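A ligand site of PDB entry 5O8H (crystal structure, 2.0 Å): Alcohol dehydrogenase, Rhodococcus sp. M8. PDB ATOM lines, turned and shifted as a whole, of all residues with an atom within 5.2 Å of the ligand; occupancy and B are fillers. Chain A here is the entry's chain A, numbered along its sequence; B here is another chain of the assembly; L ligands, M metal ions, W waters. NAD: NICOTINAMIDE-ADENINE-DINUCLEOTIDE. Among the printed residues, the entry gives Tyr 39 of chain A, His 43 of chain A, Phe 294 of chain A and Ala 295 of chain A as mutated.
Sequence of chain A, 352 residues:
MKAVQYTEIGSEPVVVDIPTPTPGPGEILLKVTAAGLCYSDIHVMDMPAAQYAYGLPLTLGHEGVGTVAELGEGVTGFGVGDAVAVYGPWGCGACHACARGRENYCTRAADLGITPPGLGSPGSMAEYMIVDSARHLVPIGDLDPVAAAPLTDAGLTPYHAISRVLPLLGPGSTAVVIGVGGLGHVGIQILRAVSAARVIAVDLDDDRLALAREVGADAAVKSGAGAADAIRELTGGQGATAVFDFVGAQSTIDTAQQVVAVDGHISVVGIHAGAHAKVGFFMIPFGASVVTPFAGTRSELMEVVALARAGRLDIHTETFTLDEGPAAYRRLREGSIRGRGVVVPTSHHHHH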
ATOM      1  N   CYS A  38      -1.533 -17.106  19.556  1.00  0.00           N
ATOM      2  CA  CYS A  38      -0.576 -17.836  20.411  1.00  0.00           C
ATOM      3  C   CYS A  38      -0.009 -19.012  19.625  1.00  0.00           C
ATOM      4  O   CYS A  38      -0.720 -19.659  18.843  1.00  0.00           O
ATOM      5  CB  CYS A  38      -1.248 -18.374  21.656  1.00  0.00           C
ATOM      6  SG  CYS A  38      -0.055 -19.232  22.754  1.00  0.00           S
ATOM      7  N   TYR A  39       1.268 -19.320  19.873  1.00  0.00           N
ATOM      8  CA  TYR A  39       1.911 -20.409  19.155  1.00  0.00           C
ATOM      9  C   TYR A  39       1.231 -21.756  19.434  1.00  0.00           C
ATOM     10  O   TYR A  39       1.316 -22.687  18.630  1.00  0.00           O
ATOM     11  CB  TYR A  39       3.431 -20.456  19.412  1.00  0.00           C
ATOM     12  CG  TYR A  39       4.166 -21.258  18.374  1.00  0.00           C
ATOM     13  CD1 TYR A  39       4.322 -22.635  18.525  1.00  0.00           C
ATOM     14  CD2 TYR A  39       4.673 -20.669  17.223  1.00  0.00           C
ATOM     15  CE1 TYR A  39       4.993 -23.385  17.560  1.00  0.00           C
ATOM     16  CE2 TYR A  39       5.320 -21.423  16.256  1.00  0.00           C
ATOM     17  CZ  TYR A  39       5.468 -22.794  16.444  1.00  0.00           C
ATOM     18  OH  TYR A  39       6.111 -23.577  15.523  1.00  0.00           O
ATOM     19  N   SER A  40       0.502 -21.852  20.554  1.00  0.00           N
ATOM     20  CA  SER A  40      -0.336 -23.020  20.816  1.00  0.00           C
ATOM     21  C   SER A  40      -1.356 -23.286  19.696  1.00  0.00           C
ATOM     22  O   SER A  40      -1.691 -24.443  19.440  1.00  0.00           O
ATOM     23  CB  SER A  40      -1.050 -22.906  22.165  1.00  0.00           C
ATOM     24  OG  SER A  40      -0.098 -23.022  23.237  1.00  0.00           O
ATOM     25  N   HIS A  43       0.405 -25.473  17.278  1.00  0.00           N
ATOM     26  CA  HIS A  43       0.412 -26.873  17.766  1.00  0.00           C
ATOM     27  C   HIS A  43      -0.925 -27.532  17.408  1.00  0.00           C
ATOM     28  O   HIS A  43      -0.939 -28.635  16.874  1.00  0.00           O
ATOM     29  CB  HIS A  43       0.661 -26.999  19.284  1.00  0.00           C
ATOM     30  CG  HIS A  43       2.012 -26.512  19.728  1.00  0.00           C
ATOM     31  ND1 HIS A  43       3.182 -26.823  19.081  1.00  0.00           N
ATOM     32  CD2 HIS A  43       2.363 -25.732  20.787  1.00  0.00           C
ATOM     33  CE1 HIS A  43       4.198 -26.263  19.709  1.00  0.00           C
ATOM     34  NE2 HIS A  43       3.731 -25.597  20.750  1.00  0.00           N
ATOM     35  N   ASP A 153      -3.057 -14.750  28.108  1.00  0.00           N
ATOM     36  CA  ASP A 153      -2.280 -15.987  28.052  1.00  0.00           C
ATOM     37  C   ASP A 153      -0.768 -15.764  28.059  1.00  0.00           C
ATOM     38  O   ASP A 153      -0.058 -16.320  28.904  1.00  0.00           O
ATOM     39  CB  ASP A 153      -2.738 -16.847  26.882  1.00  0.00           C
ATOM     40  CG  ASP A 153      -2.379 -18.310  27.037  1.00  0.00           C
ATOM     41  OD1 ASP A 153      -2.206 -18.861  28.164  1.00  0.00           O
ATOM     42  OD2 ASP A 153      -2.320 -18.921  25.981  1.00  0.00           O
ATOM     43  N   THR A 157       0.096 -17.038  31.688  1.00  0.00           N
ATOM     44  CA  THR A 157       0.839 -18.273  31.816  1.00  0.00           C
ATOM     45  C   THR A 157       2.214 -18.088  32.501  1.00  0.00           C
ATOM     46  O   THR A 157       2.504 -18.808  33.479  1.00  0.00           O
ATOM     47  CB  THR A 157       0.920 -19.022  30.471  1.00  0.00           C
ATOM     48  OG1 THR A 157      -0.401 -19.426  30.112  1.00  0.00           O
ATOM     49  CG2 THR A 157       1.783 -20.242  30.575  1.00  0.00           C
ATOM     50  N   ILE A 178      14.112 -18.685  29.175  1.00  0.00           N
ATOM     51  CA  ILE A 178      14.483 -19.235  27.878  1.00  0.00           C
ATOM     52  C   ILE A 178      13.345 -19.042  26.903  1.00  0.00           C
ATOM     53  O   ILE A 178      12.251 -19.543  27.106  1.00  0.00           O
ATOM     54  CB  ILE A 178      14.883 -20.709  27.927  1.00  0.00           C
ATOM     55  CG1 ILE A 178      15.930 -20.945  29.047  1.00  0.00           C
ATOM     56  CG2 ILE A 178      15.485 -21.134  26.572  1.00  0.00           C
ATOM     57  CD1 ILE A 178      16.366 -22.389  29.189  1.00  0.00           C
ATOM     58  N   GLY A 179      13.603 -18.280  25.843  1.00  0.00           N
ATOM     59  CA  GLY A 179      12.617 -17.986  24.815  1.00  0.00           C
ATOM     60  C   GLY A 179      11.991 -16.647  25.052  1.00  0.00           C
ATOM     61  O   GLY A 179      11.141 -16.498  25.938  1.00  0.00           O
ATOM     62  N   VAL A 180      12.412 -15.646  24.279  1.00  0.00           N
ATOM     63  CA  VAL A 180      11.915 -14.275  24.416  1.00  0.00           C
ATOM     64  C   VAL A 180      10.933 -13.908  23.276  1.00  0.00           C
ATOM     65  O   VAL A 180      11.196 -13.021  22.454  1.00  0.00           O
ATOM     66  CB  VAL A 180      13.089 -13.277  24.492  1.00  0.00           C
ATOM     67  CG1 VAL A 180      12.598 -11.890  24.940  1.00  0.00           C
ATOM     68  CG2 VAL A 180      14.142 -13.773  25.471  1.00  0.00           C
ATOM     69  N   GLY A 181       9.803 -14.595  23.265  1.00  0.00           N
ATOM     70  CA  GLY A 181       8.713 -14.351  22.315  1.00  0.00           C
ATOM     71  C   GLY A 181       7.511 -13.770  23.018  1.00  0.00           C
ATOM     72  O   GLY A 181       7.664 -12.962  23.937  1.00  0.00           O
ATOM     73  N   GLY A 182       6.312 -14.201  22.599  1.00  0.00           N
ATOM     74  CA  GLY A 182       5.090 -13.727  23.193  1.00  0.00           C
ATOM     75  C   GLY A 182       5.091 -13.857  24.707  1.00  0.00           C
ATOM     76  O   GLY A 182       4.949 -12.861  25.436  1.00  0.00           O
ATOM     77  N   LEU A 183       5.299 -15.081  25.175  1.00  0.00           N
ATOM     78  CA  LEU A 183       5.313 -15.364  26.612  1.00  0.00           C
ATOM     79  C   LEU A 183       6.556 -14.799  27.287  1.00  0.00           C
ATOM     80  O   LEU A 183       6.456 -14.070  28.292  1.00  0.00           O
ATOM     81  CB  LEU A 183       5.199 -16.873  26.926  1.00  0.00           C
ATOM     82  CG  LEU A 183       3.790 -17.423  27.078  1.00  0.00           C
ATOM     83  CD1 LEU A 183       2.993 -17.404  25.783  1.00  0.00           C
ATOM     84  CD2 LEU A 183       3.810 -18.819  27.646  1.00  0.00           C
ATOM     85  N   GLY A 184       7.714 -15.153  26.748  1.00  0.00           N
ATOM     86  CA  GLY A 184       8.985 -14.821  27.394  1.00  0.00           C
ATOM     87  C   GLY A 184       9.229 -13.332  27.659  1.00  0.00           C
ATOM     88  O   GLY A 184       9.755 -12.960  28.720  1.00  0.00           O
ATOM     89  N   VAL A 202      17.526 -15.871  27.434  1.00  0.00           N
ATOM     90  CA  VAL A 202      18.190 -16.790  26.497  1.00  0.00           C
ATOM     91  C   VAL A 202      17.329 -16.897  25.245  1.00  0.00           C
ATOM     92  O   VAL A 202      16.132 -17.137  25.346  1.00  0.00           O
ATOM     93  CB  VAL A 202      18.397 -18.192  27.120  1.00  0.00           C
ATOM     94  CG1 VAL A 202      19.117 -19.134  26.155  1.00  0.00           C
ATOM     95  CG2 VAL A 202      19.166 -18.113  28.433  1.00  0.00           C
ATOM     96  N   ASP A 203      17.928 -16.726  24.068  1.00  0.00           N
ATOM     97  CA  ASP A 203      17.188 -16.925  22.814  1.00  0.00           C
ATOM     98  C   ASP A 203      18.161 -17.255  21.684  1.00  0.00           C
ATOM     99  O   ASP A 203      19.379 -17.014  21.799  1.00  0.00           O
ATOM    100  CB  ASP A 203      16.326 -15.684  22.484  1.00  0.00           C
ATOM    101  CG  ASP A 203      15.141 -16.006  21.567  1.00  0.00           C
ATOM    102  OD1 ASP A 203      15.348 -16.392  20.401  1.00  0.00           O
ATOM    103  OD2 ASP A 203      13.985 -15.826  21.998  1.00  0.00           O
ATOM    104  N   LEU A 204      17.636 -17.870  20.634  1.00  0.00           N
ATOM    105  CA  LEU A 204      18.431 -18.200  19.426  1.00  0.00           C
ATOM    106  C   LEU A 204      18.747 -16.963  18.605  1.00  0.00           C
ATOM    107  O   LEU A 204      19.800 -16.883  17.986  1.00  0.00           O
ATOM    108  CB  LEU A 204      17.691 -19.216  18.550  1.00  0.00           C
ATOM    109  CG  LEU A 204      17.694 -20.669  19.038  1.00  0.00           C
ATOM    110  CD1 LEU A 204      16.753 -21.527  18.196  1.00  0.00           C
ATOM    111  CD2 LEU A 204      19.112 -21.276  19.027  1.00  0.00           C
ATOM    112  N   ASP A 205      17.821 -16.000  18.642  1.00  0.00           N
ATOM    113  CA  ASP A 205      17.820 -14.839  17.751  1.00  0.00           C
ATOM    114  C   ASP A 205      18.374 -13.594  18.486  1.00  0.00           C
ATOM    115  O   ASP A 205      17.848 -13.177  19.525  1.00  0.00           O
ATOM    116  CB  ASP A 205      16.371 -14.633  17.291  1.00  0.00           C
ATOM    117  CG  ASP A 205      16.168 -13.449  16.338  1.00  0.00           C
ATOM    118  OD1 ASP A 205      16.975 -12.516  16.329  1.00  0.00           O
ATOM    119  OD2 ASP A 205      15.154 -13.451  15.626  1.00  0.00           O
ATOM    120  N   ARG A 208      15.934 -10.911  19.432  1.00  0.00           N
ATOM    121  CA  ARG A 208      15.123 -11.235  20.630  1.00  0.00           C
ATOM    122  C   ARG A 208      15.896 -10.992  21.907  1.00  0.00           C
ATOM    123  O   ARG A 208      15.321 -10.584  22.905  1.00  0.00           O
ATOM    124  CB  ARG A 208      14.587 -12.678  20.578  1.00  0.00           C
ATOM    125  CG  ARG A 208      13.746 -12.986  19.366  1.00  0.00           C
ATOM    126  CD  ARG A 208      12.519 -12.046  19.256  1.00  0.00           C
ATOM    127  NE  ARG A 208      11.714 -12.263  18.059  1.00  0.00           N
ATOM    128  CZ  ARG A 208      10.633 -13.054  17.952  1.00  0.00           C
ATOM    129  NH1 ARG A 208      10.122 -13.718  18.992  1.00  0.00           N
ATOM    130  NH2 ARG A 208      10.023 -13.170  16.761  1.00  0.00           N
ATOM    131  N   SER A 223      21.261 -18.907  22.948  1.00  0.00           N
ATOM    132  CA  SER A 223      20.861 -20.274  23.224  1.00  0.00           C
ATOM    133  C   SER A 223      21.773 -21.255  22.483  1.00  0.00           C
ATOM    134  O   SER A 223      22.490 -20.868  21.572  1.00  0.00           O
ATOM    135  CB  SER A 223      19.408 -20.519  22.840  1.00  0.00           C
ATOM    136  OG  SER A 223      18.863 -21.681  23.425  1.00  0.00           O
ATOM    137  N   PHE A 246      10.350 -21.253  28.283  1.00  0.00           N
ATOM    138  CA  PHE A 246       9.194 -21.005  27.414  1.00  0.00           C
ATOM    139  C   PHE A 246       9.370 -21.590  26.005  1.00  0.00           C
ATOM    140  O   PHE A 246       8.532 -21.332  25.126  1.00  0.00           O
ATOM    141  CB  PHE A 246       8.922 -19.525  27.332  1.00  0.00           C
ATOM    142  CG  PHE A 246       8.592 -18.913  28.662  1.00  0.00           C
ATOM    143  CD1 PHE A 246       7.366 -19.159  29.260  1.00  0.00           C
ATOM    144  CD2 PHE A 246       9.514 -18.096  29.325  1.00  0.00           C
ATOM    145  CE1 PHE A 246       7.063 -18.608  30.498  1.00  0.00           C
ATOM    146  CE2 PHE A 246       9.206 -17.532  30.542  1.00  0.00           C
ATOM    147  CZ  PHE A 246       7.977 -17.807  31.137  1.00  0.00           C
ATOM    148  N   VAL A 247      10.422 -22.372  25.795  1.00  0.00           N
ATOM    149  CA  VAL A 247      10.628 -23.138  24.557  1.00  0.00           C
ATOM    150  C   VAL A 247      10.228 -24.596  24.806  1.00  0.00           C
ATOM    151  O   VAL A 247       9.332 -25.139  24.153  1.00  0.00           O
ATOM    152  CB  VAL A 247      12.077 -23.048  24.076  1.00  0.00           C
ATOM    153  CG1 VAL A 247      12.273 -23.792  22.741  1.00  0.00           C
ATOM    154  CG2 VAL A 247      12.504 -21.580  23.923  1.00  0.00           C
ATOM    155  N   ALA A 249      12.030 -27.336  24.392  1.00  0.00           N
ATOM    156  CA  ALA A 249      12.638 -28.344  23.532  1.00  0.00           C
ATOM    157  C   ALA A 249      13.570 -29.147  24.418  1.00  0.00           C
ATOM    158  O   ALA A 249      13.948 -28.690  25.508  1.00  0.00           O
ATOM    159  CB  ALA A 249      13.400 -27.694  22.395  1.00  0.00           C
ATOM    160  N   SER A 251      16.706 -29.664  24.025  1.00  0.00           N
ATOM    161  CA  SER A 251      17.951 -28.922  24.223  1.00  0.00           C
ATOM    162  C   SER A 251      17.824 -27.825  25.303  1.00  0.00           C
ATOM    163  O   SER A 251      18.753 -27.613  26.066  1.00  0.00           O
ATOM    164  CB  SER A 251      18.453 -28.303  22.905  1.00  0.00           C
ATOM    165  OG  SER A 251      17.504 -27.416  22.380  1.00  0.00           O
ATOM    166  N   THR A 252      16.700 -27.143  25.367  1.00  0.00           N
ATOM    167  CA  THR A 252      16.496 -26.064  26.360  1.00  0.00           C
ATOM    168  C   THR A 252      16.263 -26.617  27.757  1.00  0.00           C
ATOM    169  O   THR A 252      16.758 -26.063  28.732  1.00  0.00           O
ATOM    170  CB  THR A 252      15.383 -25.079  25.971  1.00  0.00           C
ATOM    171  OG1 THR A 252      14.147 -25.758  25.803  1.00  0.00           O
ATOM    172  CG2 THR A 252      15.773 -24.371  24.656  1.00  0.00           C
ATOM    173  N   VAL A 269       7.480 -24.648  30.467  1.00  0.00           N
ATOM    174  CA  VAL A 269       6.242 -23.977  30.041  1.00  0.00           C
ATOM    175  C   VAL A 269       5.975 -24.176  28.557  1.00  0.00           C
ATOM    176  O   VAL A 269       4.834 -24.446  28.151  1.00  0.00           O
ATOM    177  CB  VAL A 269       6.292 -22.474  30.372  1.00  0.00           C
ATOM    178  CG1 VAL A 269       4.983 -21.811  30.012  1.00  0.00           C
ATOM    179  CG2 VAL A 269       6.628 -22.252  31.843  1.00  0.00           C
ATOM    180  N   GLY A 270       6.991 -23.994  27.735  1.00  0.00           N
ATOM    181  CA  GLY A 270       6.879 -24.262  26.296  1.00  0.00           C
ATOM    182  C   GLY A 270       6.637 -25.747  26.003  1.00  0.00           C
ATOM    183  O   GLY A 270       7.068 -26.613  26.757  1.00  0.00           O
ATOM    184  N   ILE A 271       5.944 -26.006  24.909  1.00  0.00           N
ATOM    185  CA  ILE A 271       5.476 -27.341  24.540  1.00  0.00           C
ATOM    186  C   ILE A 271       6.212 -27.810  23.281  1.00  0.00           C
ATOM    187  O   ILE A 271       6.158 -27.156  22.233  1.00  0.00           O
ATOM    188  CB  ILE A 271       3.945 -27.338  24.290  1.00  0.00           C
ATOM    189  CG1 ILE A 271       3.196 -26.872  25.555  1.00  0.00           C
ATOM    190  CG2 ILE A 271       3.452 -28.723  23.863  1.00  0.00           C
ATOM    191  CD1 ILE A 271       1.753 -26.449  25.310  1.00  0.00           C
ATOM    192  N   PRO A 293       3.630 -26.231  34.219  1.00  0.00           N
ATOM    193  CA  PRO A 293       2.448 -25.525  34.646  1.00  0.00           C
ATOM    194  C   PRO A 293       1.504 -25.283  33.463  1.00  0.00           C
ATOM    195  O   PRO A 293       1.928 -25.415  32.283  1.00  0.00           O
ATOM    196  CB  PRO A 293       2.995 -24.209  35.175  1.00  0.00           C
ATOM    197  CG  PRO A 293       4.185 -23.927  34.329  1.00  0.00           C
ATOM    198  CD  PRO A 293       4.722 -25.291  33.888  1.00  0.00           C
ATOM    199  N   PHE A 294       0.252 -24.984  33.760  1.00  0.00           N
ATOM    200  CA  PHE A 294      -0.771 -24.765  32.719  1.00  0.00           C
ATOM    201  C   PHE A 294      -1.590 -23.518  33.030  1.00  0.00           C
ATOM    202  O   PHE A 294      -2.211 -23.423  34.076  1.00  0.00           O
ATOM    203  CB  PHE A 294      -1.729 -25.934  32.586  1.00  0.00           C
ATOM    204  CG  PHE A 294      -2.756 -25.744  31.490  1.00  0.00           C
ATOM    205  CD1 PHE A 294      -2.370 -25.711  30.150  1.00  0.00           C
ATOM    206  CD2 PHE A 294      -4.101 -25.609  31.801  1.00  0.00           C
ATOM    207  CE1 PHE A 294      -3.327 -25.515  29.139  1.00  0.00           C
ATOM    208  CE2 PHE A 294      -5.056 -25.432  30.802  1.00  0.00           C
ATOM    209  CZ  PHE A 294      -4.674 -25.383  29.478  1.00  0.00           C
ATOM    210  N   ALA A 295      -1.541 -22.569  32.101  1.00  0.00           N
ATOM    211  CA  ALA A 295      -2.352 -21.378  32.112  1.00  0.00           C
ATOM    212  C   ALA A 295      -2.207 -20.647  33.457  1.00  0.00           C
ATOM    213  O   ALA A 295      -1.091 -20.492  33.911  1.00  0.00           O
ATOM    214  CB  ALA A 295      -3.798 -21.719  31.751  1.00  0.00           C
ATOM    215  N   LEU A 332       3.666 -16.033  12.362  1.00  0.00           N
ATOM    216  CA  LEU A 332       3.953 -16.689  13.634  1.00  0.00           C
ATOM    217  C   LEU A 332       4.744 -17.988  13.428  1.00  0.00           C
ATOM    218  O   LEU A 332       5.748 -18.207  14.103  1.00  0.00           O
ATOM    219  CB  LEU A 332       2.653 -16.944  14.411  1.00  0.00           C
ATOM    220  CG  LEU A 332       2.772 -17.486  15.836  1.00  0.00           C
ATOM    221  CD1 LEU A 332       3.609 -16.567  16.721  1.00  0.00           C
ATOM    222  CD2 LEU A 332       1.363 -17.697  16.397  1.00  0.00           C
ATOM    223  N   GLY A 339       7.253 -10.184  19.303  1.00  0.00           N
ATOM    224  CA  GLY A 339       6.341 -10.110  20.432  1.00  0.00           C
ATOM    225  C   GLY A 339       5.094 -10.900  20.106  1.00  0.00           C
ATOM    226  O   GLY A 339       5.186 -12.035  19.634  1.00  0.00           O
ATOM    227  N   ARG A 340       3.928 -10.277  20.309  1.00  0.00           N
ATOM    228  CA  ARG A 340       2.637 -10.910  20.079  1.00  0.00           C
ATOM    229  C   ARG A 340       1.883 -10.337  18.890  1.00  0.00           C
ATOM    230  O   ARG A 340       1.717  -9.133  18.793  1.00  0.00           O
ATOM    231  CB  ARG A 340       1.736 -10.723  21.317  1.00  0.00           C
ATOM    232  CG  ARG A 340       1.578 -11.979  22.111  1.00  0.00           C
ATOM    233  CD  ARG A 340       0.636 -12.927  21.429  1.00  0.00           C
ATOM    234  NE  ARG A 340       0.297 -14.030  22.331  1.00  0.00           N
ATOM    235  CZ  ARG A 340       1.009 -15.147  22.515  1.00  0.00           C
ATOM    236  NH1 ARG A 340       2.152 -15.379  21.862  1.00  0.00           N
ATOM    237  NH2 ARG A 340       0.540 -16.042  23.371  1.00  0.00           N
ATOM    238  N   PHE B 281       5.188 -32.400  28.884  1.00  0.00           N
ATOM    239  CA  PHE B 281       3.791 -32.400  28.494  1.00  0.00           C
ATOM    240  C   PHE B 281       3.390 -33.760  27.934  1.00  0.00           C
ATOM    241  O   PHE B 281       4.205 -34.420  27.285  1.00  0.00           O
ATOM    242  CB  PHE B 281       3.480 -31.255  27.528  1.00  0.00           C
ATOM    243  CG  PHE B 281       3.489 -29.893  28.202  1.00  0.00           C
ATOM    244  CD1 PHE B 281       2.386 -29.425  28.897  1.00  0.00           C
ATOM    245  CD2 PHE B 281       4.650 -29.121  28.184  1.00  0.00           C
ATOM    246  CE1 PHE B 281       2.441 -28.196  29.558  1.00  0.00           C
ATOM    247  CE2 PHE B 281       4.687 -27.905  28.834  1.00  0.00           C
ATOM    248  CZ  PHE B 281       3.586 -27.436  29.515  1.00  0.00           C
HETATM  249  PA  NAD L   1       6.585 -17.430  20.111  1.00  0.00           P
HETATM  250  O1A NAD L   1       6.788 -18.070  18.805  1.00  0.00           O
HETATM  251  O2A NAD L   1       6.001 -16.055  20.250  1.00  0.00           O
HETATM  252  O5B NAD L   1       8.051 -17.288  20.783  1.00  0.00           O
HETATM  253  C5B NAD L   1       9.068 -18.251  20.617  1.00  0.00           C
HETATM  254  C4B NAD L   1      10.389 -17.667  21.093  1.00  0.00           C
HETATM  255  O4B NAD L   1      11.229 -18.750  21.449  1.00  0.00           O
HETATM  256  C3B NAD L   1      11.119 -16.880  20.000  1.00  0.00           C
HETATM  257  O3B NAD L   1      11.683 -15.684  20.529  1.00  0.00           O
HETATM  258  C2B NAD L   1      12.176 -17.856  19.506  1.00  0.00           C
HETATM  259  O2B NAD L   1      13.345 -17.255  18.965  1.00  0.00           O
HETATM  260  C1B NAD L   1      12.489 -18.592  20.798  1.00  0.00           C
HETATM  261  N9A NAD L   1      13.112 -19.937  20.602  1.00  0.00           N
HETATM  262  C8A NAD L   1      12.721 -20.948  19.796  1.00  0.00           C
HETATM  263  N7A NAD L   1      13.556 -22.000  19.934  1.00  0.00           N
HETATM  264  C5A NAD L   1      14.482 -21.660  20.849  1.00  0.00           C
HETATM  265  C6A NAD L   1      15.636 -22.292  21.488  1.00  0.00           C
HETATM  266  N6A NAD L   1      16.005 -23.543  21.164  1.00  0.00           N
HETATM  267  N1A NAD L   1      16.333 -21.606  22.410  1.00  0.00           N
HETATM  268  C2A NAD L   1      15.984 -20.336  22.752  1.00  0.00           C
HETATM  269  N3A NAD L   1      14.946 -19.673  22.204  1.00  0.00           N
HETATM  270  C4A NAD L   1      14.181 -20.294  21.286  1.00  0.00           C
HETATM  271  O3  NAD L   1       5.856 -18.507  21.073  1.00  0.00           O
HETATM  272  PN  NAD L   1       4.922 -18.139  22.376  1.00  0.00           P
HETATM  273  O1N NAD L   1       3.560 -17.806  21.903  1.00  0.00           O
HETATM  274  O2N NAD L   1       5.717 -17.236  23.284  1.00  0.00           O
HETATM  275  O5D NAD L   1       4.791 -19.635  22.948  1.00  0.00           O
HETATM  276  C5D NAD L   1       5.948 -20.286  23.498  1.00  0.00           C
HETATM  277  C4D NAD L   1       5.562 -21.690  23.906  1.00  0.00           C
HETATM  278  O4D NAD L   1       4.703 -21.622  25.060  1.00  0.00           O
HETATM  279  C3D NAD L   1       4.793 -22.499  22.841  1.00  0.00           C
HETATM  280  O3D NAD L   1       5.309 -23.833  22.760  1.00  0.00           O
HETATM  281  C2D NAD L   1       3.372 -22.489  23.358  1.00  0.00           C
HETATM  282  O2D NAD L   1       2.577 -23.585  22.875  1.00  0.00           O
HETATM  283  C1D NAD L   1       3.652 -22.533  24.861  1.00  0.00           C
HETATM  284  N1N NAD L   1       2.547 -22.134  25.740  1.00  0.00           N
HETATM  285  C2N NAD L   1       2.326 -22.889  26.832  1.00  0.00           C
HETATM  286  C3N NAD L   1       1.308 -22.584  27.719  1.00  0.00           C
HETATM  287  C7N NAD L   1       1.069 -23.394  28.953  1.00  0.00           C
HETATM  288  O7N NAD L   1       0.019 -23.269  29.535  1.00  0.00           O
HETATM  289  N7N NAD L   1       2.032 -24.186  29.449  1.00  0.00           N
HETATM  290  C4N NAD L   1       0.489 -21.457  27.464  1.00  0.00           C
HETATM  291  C5N NAD L   1       0.769 -20.676  26.322  1.00  0.00           C
HETATM  292  C6N NAD L   1       1.797 -21.026  25.487  1.00  0.00           C
HETATM  293 ZN    ZN M   1      -2.022 -20.112  24.286  1.00  0.00          ZN
HETATM  294  O   HOH W   1       7.248 -17.353  16.230  1.00  0.00           O
HETATM  295  O   HOH W   2       9.562 -19.222  23.744  1.00  0.00           O
HETATM  296  O   HOH W   3       7.217 -13.971  19.035  1.00  0.00           O
HETATM  297  O   HOH W   4       3.874 -14.326  19.848  1.00  0.00           O
HETATM  298  O   HOH W   5       8.003 -23.964  22.057  1.00  0.00           O
HETATM  299  O   HOH W   6      18.478 -24.953  22.198  1.00  0.00           O
HETATM  300  O   HOH W   7       7.436 -20.784  18.773  1.00  0.00           O
HETATM  301  O   HOH W   8      14.517 -18.340  16.842  1.00  0.00           O
HETATM  302  O   HOH W   9      14.369 -25.668  19.051  1.00  0.00           O
HETATM  303  O   HOH W  10      10.123 -20.580  17.777  1.00  0.00           O
HETATM  304  O   HOH W  11       7.981 -16.793  24.391  1.00  0.00           O
HETATM  305  O   HOH W  12      -2.735 -21.949  28.639  1.00  0.00           O
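N of Tyr 39 is in hydrogen-bond range of O1N of the ligand, 3.4 Å away.
A nitrogen (N7N) of the ligand is in hydrogen-bond range of the backbone carbonyl oxygen (O) of Pro 293, at 3.1 Å.
The backbone carbonyl oxygen (O) of Val 269 sits at hydrogen-bond distance from a nitrogen (N7N) of the ligand (3.1 Å).
O1N of the ligand lies within salt-bridge range of NH1 of Arg 340 (2.8 Å).
The backbone NH (N) of Ile 271 sits at hydrogen-bond distance from an oxygen (O3D) of the ligand (3.1 Å).
The backbone carbonyl oxygen (O) of Val 180 lies within hydrogen-bond range of an oxygen (O3B) of the ligand.
N of Gly 182 lies within hydrogen-bond range of O2A of the ligand.
An oxygen (O3B) of the ligand lies within hydrogen-bond range of the backbone NH (N) of Gly 181 (3.5 Å).
A nitrogen (N1A) of the ligand sits at hydrogen-bond distance from the side-chain hydroxyl of Ser 223.
O of Ile 271 sits at hydrogen-bond distance from O3D of the ligand (3.5 Å).
An oxygen (O3B) of the ligand lies within hydrogen-bond range of the guanidinium group (NH1) of Arg 208 (2.9 Å).
OD1 of Asp 203 lies within hydrogen-bond range of O2B of the ligand.
An oxygen (O7N) of the ligand is in hydrogen-bond range of the backbone NH of Ala 295.
N of Leu 183 is in hydrogen-bond range of O2N of the ligand (2.9 Å).
OG of Ser 40 is in hydrogen-bond range of O2D of the ligand.
NE2 of His 43 sits at hydrogen-bond distance from O3D of the ligand, at 3.1 Å.
Water W1 bridges an oxygen (O1A) of the ligand and the backbone carbonyl oxygen (O) of Leu 332.
Water W4 lies within hydrogen-bond range of O of Gly 339 (2.6 Å), O2A of the ligand (2.8 Å) and NH1 of Arg 340 (2.9 Å).
Water W5 bridges the backbone carbonyl oxygen of Val 247 (2.7 Å) and an oxygen (O3D) of the ligand (2.8 Å).
Water W2 lies within hydrogen-bond range of O of Phe 246 (2.7 Å) and O4B of the ligand (2.9 Å).
Water W6 lies within hydrogen-bond range of the side-chain hydroxyl (OG) of Ser 251 (2.7 Å) and a nitrogen (N6A) of the ligand (3.0 Å).
Water W12 lies within hydrogen-bond range of the side-chain carboxylate of Asp 153 (3.2 Å) and an oxygen (O7N) of the ligand (3.2 Å).
The side-chain hydroxyl of Thr 157 lies within hydrogen-bond range of the side-chain carboxylate of Asp 153 (2.7 Å).
The backbone carbonyl oxygen (O) of Asp 203 is in hydrogen-bond range of the backbone NH (N) of Ser 223.
The side-chain carboxylate of Asp 203 sits at hydrogen-bond distance from the backbone NH of Asp 205, at 3.1 Å.
The backbone NH (N) of Gly 179 is in hydrogen-bond range of the backbone carbonyl oxygen (O) of Val 202, 2.8 Å away.
OD2 of Asp 203 is in hydrogen-bond range of N of Val 180, at 2.8 Å.
The guanidinium group of Arg 340 lies close to the side-chain sulfur of Cys 38.
The side-chain sulfur (SG) of Cys 38 sits close to the backbone NH (N) of Ser 40.
The backbone NH (N) of Phe 246 sits at hydrogen-bond distance from the backbone carbonyl oxygen (O) of Ile 178 (2.8 Å).
Merely in contact with the ligand: Cys 38, Asp 153, Thr 157, Ile 178, Gly 179, Leu 204, Phe 246, Val 247, Thr 252, Gly 270, Phe 294 and Phe 281 of chain B.
Within 4 Å of the ligand: Cys 38, Tyr 39, Ser 40, His 43, Asp 153, Thr 157, Ile 178, Gly 179, Val 180, Gly 181, Gly 182, Leu 183, Asp 203, Leu 204, Arg 208, Ser 223, Phe 246, Val 247, Thr 252, Val 269, Gly 270, Ile 271, Pro 293, Phe 294, Ala 295, Arg 340 and Phe 281 of chain B.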
